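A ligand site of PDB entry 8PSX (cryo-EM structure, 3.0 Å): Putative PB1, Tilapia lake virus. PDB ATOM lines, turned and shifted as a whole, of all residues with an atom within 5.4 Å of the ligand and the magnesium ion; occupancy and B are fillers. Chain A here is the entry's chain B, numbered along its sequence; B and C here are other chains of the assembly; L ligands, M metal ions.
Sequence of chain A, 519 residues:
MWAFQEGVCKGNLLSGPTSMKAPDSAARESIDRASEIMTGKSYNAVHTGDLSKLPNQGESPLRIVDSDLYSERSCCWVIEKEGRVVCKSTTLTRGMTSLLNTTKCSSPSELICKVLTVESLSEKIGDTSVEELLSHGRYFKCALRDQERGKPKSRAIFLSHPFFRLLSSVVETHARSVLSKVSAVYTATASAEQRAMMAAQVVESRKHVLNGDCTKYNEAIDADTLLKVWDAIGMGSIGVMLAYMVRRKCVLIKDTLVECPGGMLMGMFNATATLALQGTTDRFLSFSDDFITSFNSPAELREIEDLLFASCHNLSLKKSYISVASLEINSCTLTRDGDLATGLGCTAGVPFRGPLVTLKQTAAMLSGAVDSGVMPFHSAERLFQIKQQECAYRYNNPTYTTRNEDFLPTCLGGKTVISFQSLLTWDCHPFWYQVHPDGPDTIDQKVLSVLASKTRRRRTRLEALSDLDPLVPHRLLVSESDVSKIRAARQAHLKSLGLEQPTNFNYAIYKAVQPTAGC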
ATOM      1  N   ARG A 145     -16.453   4.326  34.577  1.00  0.00           N
ATOM      2  CA  ARG A 145     -17.436   5.400  34.554  1.00  0.00           C
ATOM      3  C   ARG A 145     -18.799   4.775  34.312  1.00  0.00           C
ATOM      4  O   ARG A 145     -19.010   4.099  33.296  1.00  0.00           O
ATOM      5  CB  ARG A 145     -17.098   6.433  33.482  1.00  0.00           C
ATOM      6  CG  ARG A 145     -18.158   7.508  33.267  1.00  0.00           C
ATOM      7  CD  ARG A 145     -17.947   8.708  34.173  1.00  0.00           C
ATOM      8  NE  ARG A 145     -18.261   9.958  33.500  1.00  0.00           N
ATOM      9  CZ  ARG A 145     -19.485  10.460  33.369  1.00  0.00           C
ATOM     10  NH1 ARG A 145     -20.540   9.829  33.856  1.00  0.00           N
ATOM     11  NH2 ARG A 145     -19.655  11.612  32.729  1.00  0.00           N
ATOM     12  N   GLU A 148     -24.204   6.410  33.095  1.00  0.00           N
ATOM     13  CA  GLU A 148     -24.447   6.905  31.739  1.00  0.00           C
ATOM     14  C   GLU A 148     -25.666   6.190  31.175  1.00  0.00           C
ATOM     15  O   GLU A 148     -25.636   4.964  30.994  1.00  0.00           O
ATOM     16  CB  GLU A 148     -23.230   6.685  30.847  1.00  0.00           C
ATOM     17  CG  GLU A 148     -22.026   7.530  31.206  1.00  0.00           C
ATOM     18  CD  GLU A 148     -21.070   7.709  30.049  1.00  0.00           C
ATOM     19  OE1 GLU A 148     -21.269   8.639  29.239  1.00  0.00           O
ATOM     20  OE2 GLU A 148     -20.118   6.911  29.936  1.00  0.00           O
ATOM     21  N   LYS A 151     -26.198   2.805  28.566  1.00  0.00           N
ATOM     22  CA  LYS A 151     -24.955   2.034  28.561  1.00  0.00           C
ATOM     23  C   LYS A 151     -24.969   1.067  29.735  1.00  0.00           C
ATOM     24  O   LYS A 151     -24.377   1.336  30.783  1.00  0.00           O
ATOM     25  CB  LYS A 151     -23.738   2.949  28.626  1.00  0.00           C
ATOM     26  CG  LYS A 151     -23.498   3.746  27.356  1.00  0.00           C
ATOM     27  CD  LYS A 151     -22.052   4.184  27.232  1.00  0.00           C
ATOM     28  CE  LYS A 151     -21.159   3.045  26.756  1.00  0.00           C
ATOM     29  NZ  LYS A 151     -20.690   3.238  25.364  1.00  0.00           N
ATOM     30  N   ARG A 155     -18.395   2.328  30.998  1.00  0.00           N
ATOM     31  CA  ARG A 155     -17.231   2.517  30.140  1.00  0.00           C
ATOM     32  C   ARG A 155     -15.951   2.594  30.977  1.00  0.00           C
ATOM     33  O   ARG A 155     -15.979   2.831  32.183  1.00  0.00           O
ATOM     34  CB  ARG A 155     -17.396   3.767  29.278  1.00  0.00           C
ATOM     35  CG  ARG A 155     -17.054   5.082  29.961  1.00  0.00           C
ATOM     36  CD  ARG A 155     -17.091   6.247  28.984  1.00  0.00           C
ATOM     37  NE  ARG A 155     -18.373   6.358  28.298  1.00  0.00           N
ATOM     38  CZ  ARG A 155     -18.535   6.338  26.985  1.00  0.00           C
ATOM     39  NH1 ARG A 155     -17.514   6.195  26.155  1.00  0.00           N
ATOM     40  NH2 ARG A 155     -19.759   6.469  26.482  1.00  0.00           N
ATOM     41  N   ASP A 213     -22.815   9.252  13.518  1.00  0.00           N
ATOM     42  CA  ASP A 213     -22.023   8.946  14.703  1.00  0.00           C
ATOM     43  C   ASP A 213     -20.889   8.014  14.284  1.00  0.00           C
ATOM     44  O   ASP A 213     -20.967   7.352  13.239  1.00  0.00           O
ATOM     45  CB  ASP A 213     -22.876   8.293  15.806  1.00  0.00           C
ATOM     46  CG  ASP A 213     -22.235   8.411  17.180  1.00  0.00           C
ATOM     47  OD1 ASP A 213     -22.127   9.541  17.693  1.00  0.00           O
ATOM     48  OD2 ASP A 213     -21.838   7.368  17.738  1.00  0.00           O
ATOM     49  N   CYS A 214     -19.840   7.974  15.093  1.00  0.00           N
ATOM     50  CA  CYS A 214     -18.685   7.125  14.818  1.00  0.00           C
ATOM     51  C   CYS A 214     -18.543   6.099  15.938  1.00  0.00           C
ATOM     52  O   CYS A 214     -18.890   6.360  17.100  1.00  0.00           O
ATOM     53  CB  CYS A 214     -17.393   7.928  14.694  1.00  0.00           C
ATOM     54  SG  CYS A 214     -17.478   9.293  13.509  1.00  0.00           S
ATOM     55  N   THR A 215     -18.033   4.929  15.577  1.00  0.00           N
ATOM     56  CA  THR A 215     -17.865   3.820  16.494  1.00  0.00           C
ATOM     57  C   THR A 215     -16.387   3.572  16.742  1.00  0.00           C
ATOM     58  O   THR A 215     -15.556   3.732  15.841  1.00  0.00           O
ATOM     59  CB  THR A 215     -18.525   2.548  15.941  1.00  0.00           C
ATOM     60  OG1 THR A 215     -18.419   1.492  16.897  1.00  0.00           O
ATOM     61  CG2 THR A 215     -17.882   2.125  14.623  1.00  0.00           C
ATOM     62  N   LYS A 216     -16.048   3.186  17.973  1.00  0.00           N
ATOM     63  CA  LYS A 216     -14.661   2.961  18.373  1.00  0.00           C
ATOM     64  C   LYS A 216     -13.813   4.188  18.065  1.00  0.00           C
ATOM     65  O   LYS A 216     -12.691   4.085  17.563  1.00  0.00           O
ATOM     66  CB  LYS A 216     -14.087   1.710  17.699  1.00  0.00           C
ATOM     67  CG  LYS A 216     -15.011   0.498  17.706  1.00  0.00           C
ATOM     68  CD  LYS A 216     -15.016  -0.192  19.061  1.00  0.00           C
ATOM     69  CE  LYS A 216     -16.392  -0.717  19.406  1.00  0.00           C
ATOM     70  NZ  LYS A 216     -16.929  -1.636  18.350  1.00  0.00           N
ATOM     71  N   TYR A 217     -14.357   5.359  18.364  1.00  0.00           N
ATOM     72  CA  TYR A 217     -13.711   6.609  17.979  1.00  0.00           C
ATOM     73  C   TYR A 217     -12.300   6.709  18.543  1.00  0.00           C
ATOM     74  O   TYR A 217     -11.339   6.958  17.797  1.00  0.00           O
ATOM     75  CB  TYR A 217     -14.549   7.796  18.447  1.00  0.00           C
ATOM     76  CG  TYR A 217     -14.061   9.133  17.927  1.00  0.00           C
ATOM     77  CD1 TYR A 217     -14.126   9.435  16.579  1.00  0.00           C
ATOM     78  CD2 TYR A 217     -13.540  10.087  18.790  1.00  0.00           C
ATOM     79  CE1 TYR A 217     -13.696  10.651  16.107  1.00  0.00           C
ATOM     80  CE2 TYR A 217     -13.098  11.296  18.321  1.00  0.00           C
ATOM     81  CZ  TYR A 217     -13.173  11.582  16.978  1.00  0.00           C
ATOM     82  OH  TYR A 217     -12.737  12.793  16.501  1.00  0.00           O
ATOM     83  N   ASN A 218     -12.148   6.508  19.844  1.00  0.00           N
ATOM     84  CA  ASN A 218     -10.847   6.690  20.472  1.00  0.00           C
ATOM     85  C   ASN A 218      -9.887   5.556  20.110  1.00  0.00           C
ATOM     86  O   ASN A 218      -8.673   5.750  20.137  1.00  0.00           O
ATOM     87  CB  ASN A 218     -10.995   6.797  21.989  1.00  0.00           C
ATOM     88  CG  ASN A 218     -11.429   5.499  22.625  1.00  0.00           C
ATOM     89  OD1 ASN A 218     -10.610   4.643  22.940  1.00  0.00           O
ATOM     90  ND2 ASN A 218     -12.732   5.352  22.825  1.00  0.00           N
ATOM     91  N   GLU A 219     -10.418   4.372  19.786  1.00  0.00           N
ATOM     92  CA  GLU A 219      -9.563   3.255  19.413  1.00  0.00           C
ATOM     93  C   GLU A 219      -9.021   3.392  17.999  1.00  0.00           C
ATOM     94  O   GLU A 219      -7.942   2.859  17.700  1.00  0.00           O
ATOM     95  CB  GLU A 219     -10.316   1.936  19.556  1.00  0.00           C
ATOM     96  CG  GLU A 219     -10.625   1.564  20.995  1.00  0.00           C
ATOM     97  CD  GLU A 219     -12.090   1.761  21.345  1.00  0.00           C
ATOM     98  OE1 GLU A 219     -12.443   2.884  21.774  1.00  0.00           O
ATOM     99  OE2 GLU A 219     -12.870   0.815  21.204  1.00  0.00           O
ATOM    100  N   MET A 264      -6.140   6.183  21.426  1.00  0.00           N
ATOM    101  CA  MET A 264      -5.733   7.338  22.213  1.00  0.00           C
ATOM    102  C   MET A 264      -6.352   7.336  23.614  1.00  0.00           C
ATOM    103  O   MET A 264      -6.299   8.350  24.309  1.00  0.00           O
ATOM    104  CB  MET A 264      -6.095   8.639  21.483  1.00  0.00           C
ATOM    105  CG  MET A 264      -7.583   8.848  21.249  1.00  0.00           C
ATOM    106  SD  MET A 264      -7.955  10.534  20.727  1.00  0.00           S
ATOM    107  CE  MET A 264      -9.730  10.552  20.924  1.00  0.00           C
ATOM    108  N   MET A 266      -9.641   6.887  25.009  1.00  0.00           N
ATOM    109  CA  MET A 266     -10.953   7.422  25.410  1.00  0.00           C
ATOM    110  C   MET A 266     -10.902   8.936  25.612  1.00  0.00           C
ATOM    111  O   MET A 266     -10.957   9.462  26.731  1.00  0.00           O
ATOM    112  CB  MET A 266     -11.457   6.697  26.666  1.00  0.00           C
ATOM    113  CG  MET A 266     -12.780   7.239  27.222  1.00  0.00           C
ATOM    114  SD  MET A 266     -14.278   6.513  26.508  1.00  0.00           S
ATOM    115  CE  MET A 266     -14.040   4.753  26.720  1.00  0.00           C
ATOM    116  N   GLY A 267     -10.752   9.629  24.488  1.00  0.00           N
ATOM    117  CA  GLY A 267     -10.975  11.067  24.466  1.00  0.00           C
ATOM    118  C   GLY A 267      -9.868  11.887  25.085  1.00  0.00           C
ATOM    119  O   GLY A 267     -10.150  12.923  25.698  1.00  0.00           O
ATOM    120  N   ASN A 270      -9.620  15.348  22.025  1.00  0.00           N
ATOM    121  CA  ASN A 270     -10.856  15.582  21.275  1.00  0.00           C
ATOM    122  C   ASN A 270     -10.644  16.600  20.166  1.00  0.00           C
ATOM    123  O   ASN A 270     -11.125  16.422  19.053  1.00  0.00           O
ATOM    124  CB  ASN A 270     -11.972  16.028  22.227  1.00  0.00           C
ATOM    125  CG  ASN A 270     -12.303  14.980  23.267  1.00  0.00           C
ATOM    126  OD1 ASN A 270     -12.534  13.821  22.946  1.00  0.00           O
ATOM    127  ND2 ASN A 270     -12.342  15.392  24.530  1.00  0.00           N
ATOM    128  N   SER A 288     -15.620  15.971  17.853  1.00  0.00           N
ATOM    129  CA  SER A 288     -15.422  14.604  18.345  1.00  0.00           C
ATOM    130  C   SER A 288     -16.198  13.669  17.404  1.00  0.00           C
ATOM    131  O   SER A 288     -16.131  13.849  16.180  1.00  0.00           O
ATOM    132  CB  SER A 288     -15.824  14.525  19.805  1.00  0.00           C
ATOM    133  OG  SER A 288     -15.495  13.263  20.355  1.00  0.00           O
ATOM    134  N   ASP A 289     -16.932  12.694  17.914  1.00  0.00           N
ATOM    135  CA  ASP A 289     -17.614  11.704  17.072  1.00  0.00           C
ATOM    136  C   ASP A 289     -19.100  12.050  16.917  1.00  0.00           C
ATOM    137  O   ASP A 289     -19.994  11.280  17.272  1.00  0.00           O
ATOM    138  CB  ASP A 289     -17.416  10.304  17.658  1.00  0.00           C
ATOM    139  CG  ASP A 289     -18.342   9.999  18.800  1.00  0.00           C
ATOM    140  OD1 ASP A 289     -18.673  10.932  19.567  1.00  0.00           O
ATOM    141  OD2 ASP A 289     -18.768   8.831  18.933  1.00  0.00           O
ATOM    142  N   SER A 316     -20.684   4.872  12.214  1.00  0.00           N
ATOM    143  CA  SER A 316     -21.337   3.880  13.070  1.00  0.00           C
ATOM    144  C   SER A 316     -22.609   3.432  12.372  1.00  0.00           C
ATOM    145  O   SER A 316     -23.617   4.132  12.375  1.00  0.00           O
ATOM    146  CB  SER A 316     -21.621   4.466  14.442  1.00  0.00           C
ATOM    147  OG  SER A 316     -22.447   3.597  15.203  1.00  0.00           O
ATOM    148  N   LYS A 319     -25.914   3.252  14.602  1.00  0.00           N
ATOM    149  CA  LYS A 319     -26.602   4.449  15.065  1.00  0.00           C
ATOM    150  C   LYS A 319     -26.804   5.506  13.993  1.00  0.00           C
ATOM    151  O   LYS A 319     -27.770   6.266  14.074  1.00  0.00           O
ATOM    152  CB  LYS A 319     -25.836   5.075  16.227  1.00  0.00           C
ATOM    153  CG  LYS A 319     -25.543   4.114  17.360  1.00  0.00           C
ATOM    154  CD  LYS A 319     -25.068   4.837  18.603  1.00  0.00           C
ATOM    155  CE  LYS A 319     -24.956   3.890  19.791  1.00  0.00           C
ATOM    156  NZ  LYS A 319     -24.672   4.611  21.056  1.00  0.00           N
ATOM    157  P     G B  30     -12.321  11.755  38.165  1.00  0.00           P
ATOM    158  OP1   G B  30     -11.594  12.015  39.424  1.00  0.00           O
ATOM    159  OP2   G B  30     -13.670  12.328  37.958  1.00  0.00           O
ATOM    160  O5'   G B  30     -11.393  12.237  36.960  1.00  0.00           O
ATOM    161  C5'   G B  30     -10.033  11.853  36.890  1.00  0.00           C
ATOM    162  C4'   G B  30      -9.618  11.504  35.484  1.00  0.00           C
ATOM    163  O4'   G B  30     -10.344  10.342  35.017  1.00  0.00           O
ATOM    164  C3'   G B  30      -9.896  12.568  34.429  1.00  0.00           C
ATOM    165  O3'   G B  30      -8.926  13.592  34.400  1.00  0.00           O
ATOM    166  C2'   G B  30      -9.953  11.741  33.150  1.00  0.00           C
ATOM    167  O2'   G B  30      -8.659  11.442  32.672  1.00  0.00           O
ATOM    168  C1'   G B  30     -10.617  10.463  33.641  1.00  0.00           C
ATOM    169  N9    G B  30     -12.077  10.470  33.458  1.00  0.00           N
ATOM    170  C8    G B  30     -13.022  10.438  34.443  1.00  0.00           C
ATOM    171  N7    G B  30     -14.250  10.447  33.975  1.00  0.00           N
ATOM    172  C5    G B  30     -14.080  10.495  32.599  1.00  0.00           C
ATOM    173  C6    G B  30     -15.037  10.525  31.565  1.00  0.00           C
ATOM    174  O6    G B  30     -16.277  10.524  31.657  1.00  0.00           O
ATOM    175  N1    G B  30     -14.447  10.570  30.313  1.00  0.00           N
ATOM    176  C2    G B  30     -13.094  10.575  30.083  1.00  0.00           C
ATOM    177  N2    G B  30     -12.729  10.625  28.805  1.00  0.00           N
ATOM    178  N3    G B  30     -12.181  10.549  31.038  1.00  0.00           N
ATOM    179  C4    G B  30     -12.748  10.504  32.262  1.00  0.00           C
ATOM    180  P     U B  31      -9.341  15.087  34.004  1.00  0.00           P
ATOM    181  OP1   U B  31      -8.197  15.971  34.324  1.00  0.00           O
ATOM    182  OP2   U B  31     -10.678  15.381  34.572  1.00  0.00           O
ATOM    183  O5'   U B  31      -9.507  15.030  32.418  1.00  0.00           O
ATOM    184  C5'   U B  31      -8.413  14.722  31.575  1.00  0.00           C
ATOM    185  C4'   U B  31      -8.820  14.783  30.125  1.00  0.00           C
ATOM    186  O4'   U B  31      -9.720  13.680  29.824  1.00  0.00           O
ATOM    187  C3'   U B  31      -9.601  16.020  29.715  1.00  0.00           C
ATOM    188  O3'   U B  31      -8.777  17.143  29.457  1.00  0.00           O
ATOM    189  C2'   U B  31     -10.387  15.544  28.514  1.00  0.00           C
ATOM    190  O2'   U B  31      -9.587  15.537  27.342  1.00  0.00           O
ATOM    191  C1'   U B  31     -10.703  14.099  28.899  1.00  0.00           C
ATOM    192  N1    U B  31     -12.028  13.975  29.548  1.00  0.00           N
ATOM    193  C2    U B  31     -13.137  13.940  28.733  1.00  0.00           C
ATOM    194  O2    U B  31     -13.077  14.030  27.526  1.00  0.00           O
ATOM    195  N3    U B  31     -14.335  13.813  29.404  1.00  0.00           N
ATOM    196  C4    U B  31     -14.526  13.710  30.761  1.00  0.00           C
ATOM    197  O4    U B  31     -15.656  13.600  31.203  1.00  0.00           O
ATOM    198  C5    U B  31     -13.323  13.743  31.535  1.00  0.00           C
ATOM    199  C6    U B  31     -12.144  13.874  30.915  1.00  0.00           C
ATOM    200  P     A C  21     -24.862  12.910  23.608  1.00  0.00           P
ATOM    201  OP1   A C  21     -25.513  12.429  22.362  1.00  0.00           O
ATOM    202  OP2   A C  21     -25.078  12.185  24.883  1.00  0.00           O
ATOM    203  O5'   A C  21     -23.293  12.984  23.347  1.00  0.00           O
ATOM    204  C5'   A C  21     -22.778  13.593  22.178  1.00  0.00           C
ATOM    205  C4'   A C  21     -21.273  13.498  22.109  1.00  0.00           C
ATOM    206  O4'   A C  21     -20.679  14.351  23.116  1.00  0.00           O
ATOM    207  C3'   A C  21     -20.678  12.130  22.385  1.00  0.00           C
ATOM    208  O3'   A C  21     -20.748  11.266  21.269  1.00  0.00           O
ATOM    209  C2'   A C  21     -19.243  12.476  22.795  1.00  0.00           C
ATOM    210  O2'   A C  21     -18.429  12.708  21.659  1.00  0.00           O
ATOM    211  C1'   A C  21     -19.447  13.803  23.541  1.00  0.00           C
ATOM    212  N9    A C  21     -19.461  13.627  24.999  1.00  0.00           N
ATOM    213  C8    A C  21     -20.518  13.398  25.839  1.00  0.00           C
ATOM    214  N7    A C  21     -20.173  13.280  27.103  1.00  0.00           N
ATOM    215  C5    A C  21     -18.795  13.449  27.086  1.00  0.00           C
ATOM    216  C6    A C  21     -17.820  13.425  28.097  1.00  0.00           C
ATOM    217  N6    A C  21     -18.067  13.241  29.397  1.00  0.00           N
ATOM    218  N1    A C  21     -16.533  13.617  27.730  1.00  0.00           N
ATOM    219  C2    A C  21     -16.257  13.808  26.435  1.00  0.00           C
ATOM    220  N3    A C  21     -17.087  13.839  25.399  1.00  0.00           N
ATOM    221  C4    A C  21     -18.346  13.651  25.795  1.00  0.00           C
HETATM  222  C1  LIG L   1     -18.266   9.742  26.626  1.00  0.00           C
HETATM  223  C2  LIG L   1     -17.607   9.883  25.462  1.00  0.00           C
HETATM  224  C3  LIG L   1     -15.588  10.453  26.614  1.00  0.00           C
HETATM  225  C4  LIG L   1     -17.529   9.963  27.824  1.00  0.00           C
HETATM  226  C5  LIG L   1     -15.556  10.399  24.142  1.00  0.00           C
HETATM  227  C6  LIG L   1     -14.569   9.251  23.869  1.00  0.00           C
HETATM  228  C7  LIG L   1     -15.496   8.257  23.161  1.00  0.00           C
HETATM  229  C8  LIG L   1     -16.286   9.216  22.263  1.00  0.00           C
HETATM  230  C9  LIG L   1     -17.578   8.662  21.699  1.00  0.00           C
HETATM  231  N1  LIG L   1     -16.302  10.231  25.424  1.00  0.00           N
HETATM  232  N2  LIG L   1     -16.235  10.310  27.793  1.00  0.00           N
HETATM  233  N3  LIG L   1     -18.107   9.838  29.008  1.00  0.00           N
HETATM  234  N4  LIG L   1     -18.202   5.610  22.257  1.00  0.00           N
HETATM  235  O1  LIG L   1     -14.396  10.765  26.538  1.00  0.00           O
HETATM  236  O2  LIG L   1     -20.717   3.901  21.488  1.00  0.00           O
HETATM  237  O3  LIG L   1     -20.017   6.598  23.821  1.00  0.00           O
HETATM  238  O4  LIG L   1     -14.808   7.256  22.418  1.00  0.00           O
HETATM  239  O5  LIG L   1     -13.544   9.723  23.024  1.00  0.00           O
HETATM  240  O6  LIG L   1     -16.511  10.373  23.098  1.00  0.00           O
HETATM  241  O7  LIG L   1     -18.371   8.093  22.761  1.00  0.00           O
HETATM  242  O8  LIG L   1     -20.099   7.115  21.300  1.00  0.00           O
HETATM  243  O9  LIG L   1     -16.200   4.434  21.113  1.00  0.00           O
HETATM  244  O10 LIG L   1     -17.617   6.095  19.746  1.00  0.00           O
HETATM  245  O11 LIG L   1     -18.455   3.890  20.400  1.00  0.00           O
HETATM  246  O12 LIG L   1     -20.412   4.860  19.165  1.00  0.00           O
HETATM  247  O13 LIG L   1     -20.245   2.379  19.546  1.00  0.00           O
HETATM  248  P1  LIG L   1     -19.291   6.811  22.523  1.00  0.00           P
HETATM  249  P2  LIG L   1     -17.512   5.104  20.859  1.00  0.00           P
HETATM  250  P3  LIG L   1     -20.044   3.759  20.140  1.00  0.00           P
HETATM  251 MG    MG M   1     -20.082   6.737  19.100  1.00  0.00          MG
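O3 of the ligand lies within salt-bridge range of NH2 of Arg 155, at 2.7 Å.
O6 of G 30 of chain B sits at hydrogen-bond distance from a nitrogen (N3) of the ligand, 3.3 Å away.
An oxygen (O9) of the ligand is in hydrogen-bond range of the backbone NH of Tyr 217 (3.4 Å).
The side-chain amide nitrogen of Asn 218 is in hydrogen-bond range of an oxygen (O4) of the ligand.
The side-chain hydroxyl (OG1) of Thr 215 lies within hydrogen-bond range of an oxygen (O13) of the ligand, 3.3 Å away.
The side-chain carboxylate (OE1) of Glu 148 is in hydrogen-bond range of a nitrogen (N3) of the ligand, at 3.4 Å.
The backbone NH (N) of Gly 267 sits at hydrogen-bond distance from an oxygen (O5) of the ligand, 3.2 Å away.
N6 of A 21 of chain C is in hydrogen-bond range of a nitrogen (N3) of the ligand (3.4 Å).
The backbone NH (N) of Lys 216 is in hydrogen-bond range of an oxygen (O9) of the ligand (3.4 Å).
The side-chain amino group of Lys 151 lies within salt-bridge range of an oxygen (O3) of the ligand (3.8 Å).
The side-chain amide oxygen (OD1) of Asn 218 is in hydrogen-bond range of the backbone NH (N) of Met 266, 3.2 Å away.
The side-chain carboxylate of Asp 289 sits close to O3' of A 21 of chain C.
The guanidinium group (NE) of Arg 145 sits at hydrogen-bond distance from O6 of G 30 of chain B, 2.8 Å away.
The backbone carbonyl oxygen (O) of Arg 155 lies within hydrogen-bond range of the backbone NH (N) of Arg 145 (2.9 Å).
O2' of A 21 of chain C is in hydrogen-bond range of OG of Ser 288 (3.3 Å).
NH1 of Arg 155 sits at hydrogen-bond distance from SD of Met 266 (3.3 Å).
The side-chain amide nitrogen of Asn 270 sits at hydrogen-bond distance from O2 of U 31 of chain B (3.4 Å).
The side-chain amide nitrogen (ND2) of Asn 218 lies within hydrogen-bond range of the side-chain carboxylate (OE1) of Glu 219, 2.7 Å away.
O of Met 266 touches O1 of the ligand (3.7 Å).
U 31 of chain B touches the ligand (O2 to O1, 3.7 Å).
Hydrophobic or aromatic side chains that line the ligand: Tyr 217 and Met 266.
The nearest printed residue that does not touch the ligand is Lys 319 (4.04 Å).
Of the 22 residues printed, 3 come within 4 Å of the magnesium ion.
The nearest printed residue that does not touch the magnesium ion is Thr 215 (4.5 Å).
The magnesium ion is bound by O12 of the ligand (1.9 Å), O8 of the ligand (2.2 Å), OD2 of Asp 213 (2.3 Å), O of Cys 214 (2.4 Å) and OD2 of Asp 289 (2.5 Å).
The magnesium ion has five donor atoms within binding distance.
Slightly farther from the magnesium ion lies an oxygen (O10) of the ligand (2.6 Å).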
